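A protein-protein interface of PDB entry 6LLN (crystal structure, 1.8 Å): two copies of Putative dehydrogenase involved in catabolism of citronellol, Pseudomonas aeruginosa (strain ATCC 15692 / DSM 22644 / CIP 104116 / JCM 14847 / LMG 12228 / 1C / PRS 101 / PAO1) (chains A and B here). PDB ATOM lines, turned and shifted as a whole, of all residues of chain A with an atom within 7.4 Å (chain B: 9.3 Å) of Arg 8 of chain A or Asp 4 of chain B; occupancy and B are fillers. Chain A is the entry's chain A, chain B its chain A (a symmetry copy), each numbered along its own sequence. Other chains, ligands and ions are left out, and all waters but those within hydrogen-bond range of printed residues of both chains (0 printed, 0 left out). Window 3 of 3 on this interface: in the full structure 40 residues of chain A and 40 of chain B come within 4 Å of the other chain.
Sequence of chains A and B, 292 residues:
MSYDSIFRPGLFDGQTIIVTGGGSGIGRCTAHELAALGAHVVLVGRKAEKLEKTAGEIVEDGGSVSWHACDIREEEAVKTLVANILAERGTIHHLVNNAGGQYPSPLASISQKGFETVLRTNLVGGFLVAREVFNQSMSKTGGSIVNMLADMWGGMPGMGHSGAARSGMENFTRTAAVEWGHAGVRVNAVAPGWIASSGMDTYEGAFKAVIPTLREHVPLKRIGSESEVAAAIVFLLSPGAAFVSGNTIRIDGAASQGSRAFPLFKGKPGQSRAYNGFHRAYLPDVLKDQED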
ATOM      1  N   SER A   5      26.166  17.694  -4.234  1.00  0.00           N
ATOM      2  CA  SER A   5      25.228  17.959  -3.158  1.00  0.00           C
ATOM      3  C   SER A   5      24.062  18.805  -3.667  1.00  0.00           C
ATOM      4  O   SER A   5      24.190  19.593  -4.605  1.00  0.00           O
ATOM      5  CB  SER A   5      25.951  18.658  -2.000  1.00  0.00           C
ATOM      6  OG  SER A   5      25.049  19.143  -1.023  1.00  0.00           O
ATOM      7  N   ILE A   6      22.899  18.623  -3.036  1.00  0.00           N
ATOM      8  CA  ILE A   6      21.761  19.485  -3.350  1.00  0.00           C
ATOM      9  C   ILE A   6      21.896  20.848  -2.701  1.00  0.00           C
ATOM     10  O   ILE A   6      21.128  21.759  -3.025  1.00  0.00           O
ATOM     11  CB  ILE A   6      20.438  18.814  -2.926  1.00  0.00           C
ATOM     12  CG1 ILE A   6      20.433  18.566  -1.411  1.00  0.00           C
ATOM     13  CG2 ILE A   6      20.221  17.511  -3.703  1.00  0.00           C
ATOM     14  CD1 ILE A   6      19.030  18.379  -0.800  1.00  0.00           C
ATOM     15  N   PHE A   7      22.853  21.016  -1.788  1.00  0.00           N
ATOM     16  CA  PHE A   7      23.000  22.232  -1.002  1.00  0.00           C
ATOM     17  C   PHE A   7      23.986  23.180  -1.671  1.00  0.00           C
ATOM     18  O   PHE A   7      24.857  22.758  -2.431  1.00  0.00           O
ATOM     19  CB  PHE A   7      23.450  21.893   0.429  1.00  0.00           C
ATOM     20  CG  PHE A   7      22.472  20.999   1.152  1.00  0.00           C
ATOM     21  CD1 PHE A   7      21.316  21.536   1.699  1.00  0.00           C
ATOM     22  CD2 PHE A   7      22.683  19.626   1.242  1.00  0.00           C
ATOM     23  CE1 PHE A   7      20.396  20.735   2.337  1.00  0.00           C
ATOM     24  CE2 PHE A   7      21.753  18.808   1.894  1.00  0.00           C
ATOM     25  CZ  PHE A   7      20.610  19.379   2.439  1.00  0.00           C
ATOM     26  N   ARG A   8      23.850  24.471  -1.377  1.00  0.00           N
ATOM     27  CA  ARG A   8      24.668  25.456  -2.076  1.00  0.00           C
ATOM     28  C   ARG A   8      26.114  25.362  -1.602  1.00  0.00           C
ATOM     29  O   ARG A   8      26.372  25.059  -0.437  1.00  0.00           O
ATOM     30  CB  ARG A   8      24.184  26.875  -1.824  1.00  0.00           C
ATOM     31  CG  ARG A   8      24.100  27.210  -0.369  1.00  0.00           C
ATOM     32  CD  ARG A   8      23.704  28.635  -0.094  1.00  0.00           C
ATOM     33  NE  ARG A   8      24.475  29.159   1.031  1.00  0.00           N
ATOM     34  CZ  ARG A   8      23.968  29.877   2.025  1.00  0.00           C
ATOM     35  NH1 ARG A   8      24.754  30.285   3.017  1.00  0.00           N
ATOM     36  NH2 ARG A   8      22.682  30.186   2.019  1.00  0.00           N
ATOM     37  N   PRO A   9      27.070  25.632  -2.488  1.00  0.00           N
ATOM     38  CA  PRO A   9      28.474  25.629  -2.060  1.00  0.00           C
ATOM     39  C   PRO A   9      28.691  26.538  -0.862  1.00  0.00           C
ATOM     40  O   PRO A   9      28.053  27.585  -0.724  1.00  0.00           O
ATOM     41  CB  PRO A   9      29.221  26.139  -3.300  1.00  0.00           C
ATOM     42  CG  PRO A   9      28.338  25.771  -4.446  1.00  0.00           C
ATOM     43  CD  PRO A   9      26.926  25.938  -3.924  1.00  0.00           C
ATOM     44  N   GLY A  10      29.599  26.110   0.019  1.00  0.00           N
ATOM     45  CA  GLY A  10      29.990  26.893   1.170  1.00  0.00           C
ATOM     46  C   GLY A  10      28.971  26.966   2.277  1.00  0.00           C
ATOM     47  O   GLY A  10      29.125  27.799   3.180  1.00  0.00           O
ATOM     48  N   LEU A  11      27.932  26.125   2.241  1.00  0.00           N
ATOM     49  CA  LEU A  11      26.871  26.231   3.237  1.00  0.00           C
ATOM     50  C   LEU A  11      27.402  26.060   4.655  1.00  0.00           C
ATOM     51  O   LEU A  11      26.861  26.659   5.591  1.00  0.00           O
ATOM     52  CB  LEU A  11      25.776  25.207   2.943  1.00  0.00           C
ATOM     53  CG  LEU A  11      24.531  25.214   3.838  1.00  0.00           C
ATOM     54  CD1 LEU A  11      23.872  26.586   3.864  1.00  0.00           C
ATOM     55  CD2 LEU A  11      23.552  24.129   3.366  1.00  0.00           C
ATOM     56  N   PHE A  12      28.445  25.255   4.845  1.00  0.00           N
ATOM     57  CA  PHE A  12      28.989  25.036   6.181  1.00  0.00           C
ATOM     58  C   PHE A  12      30.399  25.604   6.335  1.00  0.00           C
ATOM     59  O   PHE A  12      31.174  25.124   7.163  1.00  0.00           O
ATOM     60  CB  PHE A  12      28.950  23.550   6.529  1.00  0.00           C
ATOM     61  CG  PHE A  12      27.547  23.013   6.705  1.00  0.00           C
ATOM     62  CD1 PHE A  12      26.895  23.134   7.919  1.00  0.00           C
ATOM     63  CD2 PHE A  12      26.880  22.415   5.643  1.00  0.00           C
ATOM     64  CE1 PHE A  12      25.585  22.663   8.079  1.00  0.00           C
ATOM     65  CE2 PHE A  12      25.582  21.931   5.791  1.00  0.00           C
ATOM     66  CZ  PHE A  12      24.933  22.056   7.006  1.00  0.00           C
ATOM     67  N   ALA A  36      32.652  18.759   1.504  1.00  0.00           N
ATOM     68  CA  ALA A  36      32.449  19.402   0.205  1.00  0.00           C
ATOM     69  C   ALA A  36      31.716  20.729   0.349  1.00  0.00           C
ATOM     70  O   ALA A  36      31.887  21.627  -0.481  1.00  0.00           O
ATOM     71  CB  ALA A  36      31.688  18.468  -0.729  1.00  0.00           C
ATOM     72  N   LEU A  37      30.913  20.881   1.395  1.00  0.00           N
ATOM     73  CA  LEU A  37      30.186  22.114   1.643  1.00  0.00           C
ATOM     74  C   LEU A  37      30.966  23.080   2.518  1.00  0.00           C
ATOM     75  O   LEU A  37      30.421  24.116   2.911  1.00  0.00           O
ATOM     76  CB  LEU A  37      28.822  21.811   2.268  1.00  0.00           C
ATOM     77  CG  LEU A  37      27.880  20.983   1.382  1.00  0.00           C
ATOM     78  CD1 LEU A  37      26.655  20.513   2.171  1.00  0.00           C
ATOM     79  CD2 LEU A  37      27.437  21.785   0.160  1.00  0.00           C
ATOM     80  N   GLY A  38      32.224  22.769   2.828  1.00  0.00           N
ATOM     81  CA  GLY A  38      33.097  23.707   3.498  1.00  0.00           C
ATOM     82  C   GLY A  38      33.313  23.457   4.972  1.00  0.00           C
ATOM     83  O   GLY A  38      34.098  24.181   5.592  1.00  0.00           O
ATOM     84  N   PRO A 239      20.766  25.721   8.204  1.00  0.00           N
ATOM     85  CA  PRO A 239      19.856  26.787   8.645  1.00  0.00           C
ATOM     86  C   PRO A 239      18.416  26.550   8.242  1.00  0.00           C
ATOM     87  O   PRO A 239      17.508  27.084   8.889  1.00  0.00           O
ATOM     88  CB  PRO A 239      20.421  28.040   7.962  1.00  0.00           C
ATOM     89  CG  PRO A 239      21.850  27.727   7.715  1.00  0.00           C
ATOM     90  CD  PRO A 239      21.904  26.253   7.429  1.00  0.00           C
ATOM     91  N   TYR B   3      15.905  34.944  -3.231  1.00  0.00           N
ATOM     92  CA  TYR B   3      15.704  34.100  -2.048  1.00  0.00           C
ATOM     93  C   TYR B   3      17.050  33.542  -1.598  1.00  0.00           C
ATOM     94  O   TYR B   3      17.803  32.989  -2.400  1.00  0.00           O
ATOM     95  CB  TYR B   3      14.708  32.969  -2.352  1.00  0.00           C
ATOM     96  CG  TYR B   3      14.039  32.374  -1.127  1.00  0.00           C
ATOM     97  CD1 TYR B   3      14.708  31.460  -0.316  1.00  0.00           C
ATOM     98  CD2 TYR B   3      12.738  32.721  -0.785  1.00  0.00           C
ATOM     99  CE1 TYR B   3      14.100  30.919   0.799  1.00  0.00           C
ATOM    100  CE2 TYR B   3      12.118  32.178   0.327  1.00  0.00           C
ATOM    101  CZ  TYR B   3      12.807  31.282   1.121  1.00  0.00           C
ATOM    102  OH  TYR B   3      12.202  30.739   2.237  1.00  0.00           O
ATOM    103  N   ASP B   4      17.357  33.702  -0.309  1.00  0.00           N
ATOM    104  CA  ASP B   4      18.588  33.165   0.266  1.00  0.00           C
ATOM    105  C   ASP B   4      18.327  31.726   0.694  1.00  0.00           C
ATOM    106  O   ASP B   4      18.105  31.420   1.866  1.00  0.00           O
ATOM    107  CB  ASP B   4      19.057  34.022   1.432  1.00  0.00           C
ATOM    108  CG  ASP B   4      20.392  33.571   1.976  1.00  0.00           C
ATOM    109  OD1 ASP B   4      21.142  32.923   1.219  1.00  0.00           O
ATOM    110  OD2 ASP B   4      20.689  33.858   3.156  1.00  0.00           O
ATOM    111  N   SER B   5      18.367  30.830  -0.283  1.00  0.00           N
ATOM    112  CA  SER B   5      18.055  29.430  -0.056  1.00  0.00           C
ATOM    113  C   SER B   5      19.311  28.666   0.359  1.00  0.00           C
ATOM    114  O   SER B   5      20.435  29.014  -0.006  1.00  0.00           O
ATOM    115  CB  SER B   5      17.437  28.825  -1.323  1.00  0.00           C
ATOM    116  OG  SER B   5      17.319  27.417  -1.240  1.00  0.00           O
ATOM    117  N   ILE B   6      19.108  27.609   1.150  1.00  0.00           N
ATOM    118  CA  ILE B   6      20.225  26.729   1.485  1.00  0.00           C
ATOM    119  C   ILE B   6      20.569  25.799   0.338  1.00  0.00           C
ATOM    120  O   ILE B   6      21.609  25.136   0.379  1.00  0.00           O
ATOM    121  CB  ILE B   6      19.916  25.919   2.761  1.00  0.00           C
ATOM    122  CG1 ILE B   6      18.676  25.039   2.540  1.00  0.00           C
ATOM    123  CG2 ILE B   6      19.726  26.854   3.961  1.00  0.00           C
ATOM    124  CD1 ILE B   6      18.560  23.848   3.512  1.00  0.00           C
ATOM    125  N   PHE B   7      19.722  25.730  -0.689  1.00  0.00           N
ATOM    126  CA  PHE B   7      19.871  24.784  -1.784  1.00  0.00           C
ATOM    127  C   PHE B   7      20.635  25.423  -2.937  1.00  0.00           C
ATOM    128  O   PHE B   7      20.644  26.643  -3.093  1.00  0.00           O
ATOM    129  CB  PHE B   7      18.495  24.282  -2.250  1.00  0.00           C
ATOM    130  CG  PHE B   7      17.723  23.590  -1.152  1.00  0.00           C
ATOM    131  CD1 PHE B   7      18.028  22.280  -0.812  1.00  0.00           C
ATOM    132  CD2 PHE B   7      16.737  24.260  -0.434  1.00  0.00           C
ATOM    133  CE1 PHE B   7      17.357  21.639   0.206  1.00  0.00           C
ATOM    134  CE2 PHE B   7      16.048  23.610   0.597  1.00  0.00           C
ATOM    135  CZ  PHE B   7      16.371  22.295   0.907  1.00  0.00           C
ATOM    136  N   ARG B   8      21.273  24.586  -3.752  1.00  0.00           N
ATOM    137  CA  ARG B   8      22.133  25.123  -4.801  1.00  0.00           C
ATOM    138  C   ARG B   8      21.284  25.759  -5.896  1.00  0.00           C
ATOM    139  O   ARG B   8      20.180  25.294  -6.180  1.00  0.00           O
ATOM    140  CB  ARG B   8      22.989  24.042  -5.440  1.00  0.00           C
ATOM    141  CG  ARG B   8      22.182  22.899  -5.967  1.00  0.00           C
ATOM    142  CD  ARG B   8      22.998  21.854  -6.679  1.00  0.00           C
ATOM    143  NE  ARG B   8      22.278  21.377  -7.858  1.00  0.00           N
ATOM    144  CZ  ARG B   8      22.172  20.104  -8.214  1.00  0.00           C
ATOM    145  NH1 ARG B   8      21.472  19.772  -9.294  1.00  0.00           N
ATOM    146  NH2 ARG B   8      22.770  19.170  -7.492  1.00  0.00           N
ATOM    147  N   PRO B   9      21.789  26.814  -6.531  1.00  0.00           N
ATOM    148  CA  PRO B   9      21.043  27.414  -7.644  1.00  0.00           C
ATOM    149  C   PRO B   9      20.684  26.376  -8.695  1.00  0.00           C
ATOM    150  O   PRO B   9      21.437  25.434  -8.953  1.00  0.00           O
ATOM    151  CB  PRO B   9      22.017  28.464  -8.195  1.00  0.00           C
ATOM    152  CG  PRO B   9      22.883  28.817  -7.032  1.00  0.00           C
ATOM    153  CD  PRO B   9      23.053  27.524  -6.262  1.00  0.00           C
ATOM    154  N   GLY B  10      19.503  26.556  -9.291  1.00  0.00           N
ATOM    155  CA  GLY B  10      19.045  25.713 -10.372  1.00  0.00           C
ATOM    156  C   GLY B  10      18.615  24.325  -9.971  1.00  0.00           C
ATOM    157  O   GLY B  10      18.441  23.473 -10.852  1.00  0.00           O
ATOM    158  N   LEU B  11      18.440  24.065  -8.671  1.00  0.00           N
ATOM    159  CA  LEU B  11      18.123  22.711  -8.233  1.00  0.00           C
ATOM    160  C   LEU B  11      16.835  22.194  -8.862  1.00  0.00           C
ATOM    161  O   LEU B  11      16.707  20.989  -9.102  1.00  0.00           O
ATOM    162  CB  LEU B  11      18.036  22.662  -6.709  1.00  0.00           C
ATOM    163  CG  LEU B  11      17.788  21.300  -6.049  1.00  0.00           C
ATOM    164  CD1 LEU B  11      18.831  20.277  -6.474  1.00  0.00           C
ATOM    165  CD2 LEU B  11      17.754  21.468  -4.523  1.00  0.00           C
ATOM    166  N   CYS B  29       5.613  31.620   0.472  1.00  0.00           N
ATOM    167  CA  CYS B  29       7.040  31.553   0.763  1.00  0.00           C
ATOM    168  C   CYS B  29       7.688  30.403   0.011  1.00  0.00           C
ATOM    169  O   CYS B  29       8.759  30.563  -0.580  1.00  0.00           O
ATOM    170  CB  CYS B  29       7.257  31.403   2.268  1.00  0.00           C
ATOM    171  SG  CYS B  29       8.997  31.521   2.717  1.00  0.00           S
ATOM    172  N   HIS B  32       8.003  31.065  -3.736  1.00  0.00           N
ATOM    173  CA  HIS B  32       9.127  31.967  -3.991  1.00  0.00           C
ATOM    174  C   HIS B  32      10.454  31.225  -3.955  1.00  0.00           C
ATOM    175  O   HIS B  32      11.304  31.417  -4.833  1.00  0.00           O
ATOM    176  CB  HIS B  32       9.135  33.105  -2.970  1.00  0.00           C
ATOM    177  CG  HIS B  32       8.421  34.336  -3.426  1.00  0.00           C
ATOM    178  ND1 HIS B  32       8.998  35.268  -4.262  1.00  0.00           N
ATOM    179  CD2 HIS B  32       7.173  34.792  -3.158  1.00  0.00           C
ATOM    180  CE1 HIS B  32       8.135  36.240  -4.495  1.00  0.00           C
ATOM    181  NE2 HIS B  32       7.021  35.975  -3.837  1.00  0.00           N
ATOM    182  N   GLU B  33      10.671  30.386  -2.930  1.00  0.00           N
ATOM    183  CA  GLU B  33      11.937  29.655  -2.873  1.00  0.00           C
ATOM    184  C   GLU B  33      12.083  28.705  -4.053  1.00  0.00           C
ATOM    185  O   GLU B  33      13.160  28.611  -4.653  1.00  0.00           O
ATOM    186  CB  GLU B  33      12.074  28.877  -1.558  1.00  0.00           C
ATOM    187  CG  GLU B  33      13.435  28.213  -1.457  1.00  0.00           C
ATOM    188  CD  GLU B  33      13.741  27.626  -0.088  1.00  0.00           C
ATOM    189  OE1 GLU B  33      12.850  27.617   0.790  1.00  0.00           O
ATOM    190  OE2 GLU B  33      14.893  27.168   0.104  1.00  0.00           O
ATOM    191  N   ALA B  36      12.900  30.687  -7.080  1.00  0.00           N
ATOM    192  CA  ALA B  36      14.295  31.125  -7.022  1.00  0.00           C
ATOM    193  C   ALA B  36      15.248  29.999  -7.396  1.00  0.00           C
ATOM    194  O   ALA B  36      16.350  30.255  -7.891  1.00  0.00           O
ATOM    195  CB  ALA B  36      14.618  31.663  -5.633  1.00  0.00           C
ATOM    196  N   LEU B  37      14.845  28.752  -7.185  1.00  0.00           N
ATOM    197  CA  LEU B  37      15.663  27.602  -7.528  1.00  0.00           C
ATOM    198  C   LEU B  37      15.396  27.101  -8.937  1.00  0.00           C
ATOM    199  O   LEU B  37      15.930  26.056  -9.319  1.00  0.00           O
ATOM    200  CB  LEU B  37      15.451  26.476  -6.513  1.00  0.00           C
ATOM    201  CG  LEU B  37      15.863  26.823  -5.075  1.00  0.00           C
ATOM    202  CD1 LEU B  37      15.386  25.750  -4.093  1.00  0.00           C
ATOM    203  CD2 LEU B  37      17.376  26.993  -4.968  1.00  0.00           C
ATOM    204  N   THR B 202      14.929  31.795  13.302  1.00  0.00           N
ATOM    205  CA  THR B 202      15.969  32.779  13.103  1.00  0.00           C
ATOM    206  C   THR B 202      16.592  32.595  11.724  1.00  0.00           C
ATOM    207  O   THR B 202      17.474  33.364  11.332  1.00  0.00           O
ATOM    208  CB  THR B 202      17.061  32.697  14.192  1.00  0.00           C
ATOM    209  OG1 THR B 202      17.615  31.377  14.236  1.00  0.00           O
ATOM    210  CG2 THR B 202      16.491  33.054  15.557  1.00  0.00           C
ATOM    211  N   TYR B 203      16.147  31.576  10.985  1.00  0.00           N
ATOM    212  CA  TYR B 203      16.461  31.491   9.564  1.00  0.00           C
ATOM    213  C   TYR B 203      15.369  32.200   8.775  1.00  0.00           C
ATOM    214  O   TYR B 203      14.177  31.935   8.969  1.00  0.00           O
ATOM    215  CB  TYR B 203      16.594  30.048   9.077  1.00  0.00           C
ATOM    216  CG  TYR B 203      16.631  29.953   7.560  1.00  0.00           C
ATOM    217  CD1 TYR B 203      17.599  30.633   6.820  1.00  0.00           C
ATOM    218  CD2 TYR B 203      15.684  29.207   6.863  1.00  0.00           C
ATOM    219  CE1 TYR B 203      17.631  30.556   5.420  1.00  0.00           C
ATOM    220  CE2 TYR B 203      15.711  29.124   5.469  1.00  0.00           C
ATOM    221  CZ  TYR B 203      16.677  29.802   4.754  1.00  0.00           C
ATOM    222  OH  TYR B 203      16.689  29.712   3.372  1.00  0.00           O
ATOM    223  N   GLU B 204      15.780  33.103   7.881  1.00  0.00           N
ATOM    224  CA  GLU B 204      14.853  33.916   7.095  1.00  0.00           C
ATOM    225  C   GLU B 204      15.415  34.060   5.683  1.00  0.00           C
ATOM    226  O   GLU B 204      15.950  35.107   5.312  1.00  0.00           O
ATOM    227  CB  GLU B 204      14.640  35.280   7.740  1.00  0.00           C
ATOM    228  CG  GLU B 204      13.239  35.781   7.618  1.00  0.00           C
ATOM    229  CD  GLU B 204      12.414  35.362   8.797  1.00  0.00           C
ATOM    230  OE1 GLU B 204      13.017  34.967   9.817  1.00  0.00           O
ATOM    231  OE2 GLU B 204      11.173  35.420   8.708  1.00  0.00           O
ATOM    232  N   GLY B 205      15.291  32.997   4.887  1.00  0.00           N
ATOM    233  CA  GLY B 205      15.762  33.067   3.516  1.00  0.00           C
ATOM    234  C   GLY B 205      14.918  33.979   2.650  1.00  0.00           C
ATOM    235  O   GLY B 205      15.415  34.547   1.671  1.00  0.00           O
ATOM    236  N   ALA B 206      13.643  34.140   2.998  1.00  0.00           N
ATOM    237  CA  ALA B 206      12.720  34.971   2.232  1.00  0.00           C
ATOM    238  C   ALA B 206      13.136  36.443   2.248  1.00  0.00           C
ATOM    239  O   ALA B 206      13.399  37.026   1.188  1.00  0.00           O
ATOM    240  CB  ALA B 206      11.300  34.815   2.770  1.00  0.00           C
ATOM    241  N   SER B 227      10.032  30.805   6.219  1.00  0.00           N
ATOM    242  CA  SER B 227      11.196  30.212   5.572  1.00  0.00           C
ATOM    243  C   SER B 227      11.589  28.894   6.220  1.00  0.00           C
ATOM    244  O   SER B 227      12.131  28.000   5.548  1.00  0.00           O
ATOM    245  CB  SER B 227      12.379  31.185   5.652  1.00  0.00           C
ATOM    246  OG  SER B 227      12.289  32.185   4.660  1.00  0.00           O
ATOM    247  N   GLU B 228      11.364  28.776   7.532  1.00  0.00           N
ATOM    248  CA  GLU B 228      11.734  27.574   8.265  1.00  0.00           C
ATOM    249  C   GLU B 228      10.786  26.414   7.979  1.00  0.00           C
ATOM    250  O   GLU B 228      11.157  25.260   8.213  1.00  0.00           O
ATOM    251  CB  GLU B 228      11.806  27.905   9.761  1.00  0.00           C
ATOM    252  CG  GLU B 228      13.083  28.695  10.102  1.00  0.00           C
ATOM    253  CD  GLU B 228      13.104  29.303  11.498  1.00  0.00           C
ATOM    254  OE1 GLU B 228      12.032  29.464  12.121  1.00  0.00           O
ATOM    255  OE2 GLU B 228      14.219  29.645  11.966  1.00  0.00           O
ATOM    256  N   ALA B 231      11.803  25.538   3.755  1.00  0.00           N
ATOM    257  CA  ALA B 231      13.022  24.788   3.481  1.00  0.00           C
ATOM    258  C   ALA B 231      12.801  23.290   3.668  1.00  0.00           C
ATOM    259  O   ALA B 231      13.368  22.479   2.926  1.00  0.00           O
ATOM    260  CB  ALA B 231      14.174  25.292   4.359  1.00  0.00           C
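Hydrophobic or aromatic side chains of chain A within 4 Å of the printed part of chain B: Ile 6, Phe 7, Leu 11 and Pro 239.
Of the 22 printed residues of chain B, 7 touch a printed residue of chain A.
Among the printed residues, Asp or Glu carboxylates within 4 Å of a Lys or Arg side-chain nitrogen of the other chain: Arg 8 of chain A with Asp 4 of chain B (3.2 Å).
Asp 4 of chain B touches one residue of chain A.
Gly 10 of chain A touches none of the printed residues of chain B.
Of the printed residues of chain B, Leu 11 of chain A touches Ile 6 (3.7 Å).
Of the printed residues of chain A, Tyr 203 of chain B touches Pro 239 (3.1 Å).
Printed residues of chain A within 4 Å of Ser 5 of chain B: Arg 8 (3.2 Å).
Of the printed residues of chain B, Pro 239 of chain A touches Tyr 203.
Gly 10 of chain B touches none of the printed residues of chain A.
The nearest residue of chain A that does not touch Asp 4 of chain B is Pro 239 of chain A (7.3 Å).
The nearest printed residue of chain B that does not touch Phe 7 of chain A is Leu 11 of chain B (5.8 Å).
Phe 7 of chain B touches Ile 6 of chain A.
O of Ile 6 of chain A touches CD2 of Leu 11 of chain B (3.7 Å).
Ile 6 of chain B touches Phe 7 of chain A.
Phe 7 of chain B touches Phe 7 of chain A (CE1 to CE1, 3.8 Å).
Arg 8 of chain B touches Phe 7 of chain A.
C of Phe 7 of chain B touches N of Arg 8 of chain A, at 3.7 Å.
Arg 8 of chain A touches Arg 8 of chain B.
Ile 6 of chain B touches Leu 11 of chain A (O to CD2, 3.7 Å).
CB of Tyr 203 of chain B touches O of Pro 239 of chain A, 3.1 Å away.
The backbone carbonyl oxygen (O) of Asp 4 of chain B sits at hydrogen-bond distance from the side-chain hydroxyl (OH) of Tyr 203 of chain B, 2.7 Å away.
The side-chain carboxylate (OE2) of Glu 33 of chain B sits at hydrogen-bond distance from the side-chain hydroxyl (OG) of Ser 5 of chain B, 2.8 Å away.
N of Asp 4 of chain B sits at hydrogen-bond distance from O of Gly 205 of chain B (2.9 Å).
N of Leu 11 of chain A is in hydrogen-bond range of O of Leu 37 of chain A (3.3 Å).
The backbone NH (N) of Tyr 203 of chain B lies within hydrogen-bond range of the side-chain carboxylate (OE2) of Glu 228 of chain B, 2.9 Å away.
OG of Ser 5 of chain A sits at hydrogen-bond distance from N of Phe 7 of chain A, at 3.0 Å.
The backbone carbonyl oxygen of Ile 6 of chain B sits at hydrogen-bond distance from the backbone NH of Arg 8 of chain A (2.9 Å).
The guanidinium group (NH2) of Arg 8 of chain A lies within salt-bridge range of the side-chain carboxylate (OD1) of Asp 4 of chain B (3.2 Å).
NH2 of Arg 8 of chain B is in hydrogen-bond range of O of Ser 5 of chain A, at 3.2 Å.
The backbone carbonyl oxygen of Ser 5 of chain B is in hydrogen-bond range of the guanidinium group of Arg 8 of chain A, at 3.2 Å.
The backbone NH (N) of Arg 8 of chain B sits at hydrogen-bond distance from the backbone carbonyl oxygen (O) of Ile 6 of chain A (2.9 Å).
Ile 6 of chain A touches Leu 11 of chain B, and with the chains exchanged Leu 11 of chain A touches Ile 6 of chain B.
Phe 7 of chain A touches its own counterpart, Phe 7 of chain B.
Phe 7 of chain A touches Arg 8 of chain B, and with the chains exchanged Arg 8 of chain A touches Phe 7 of chain B.
Arg 8 of chain A touches its own counterpart, Arg 8 of chain B.
Positions printed for both chains: 5, 6, 7, 8, 9, 10, 11, 36 and 37.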
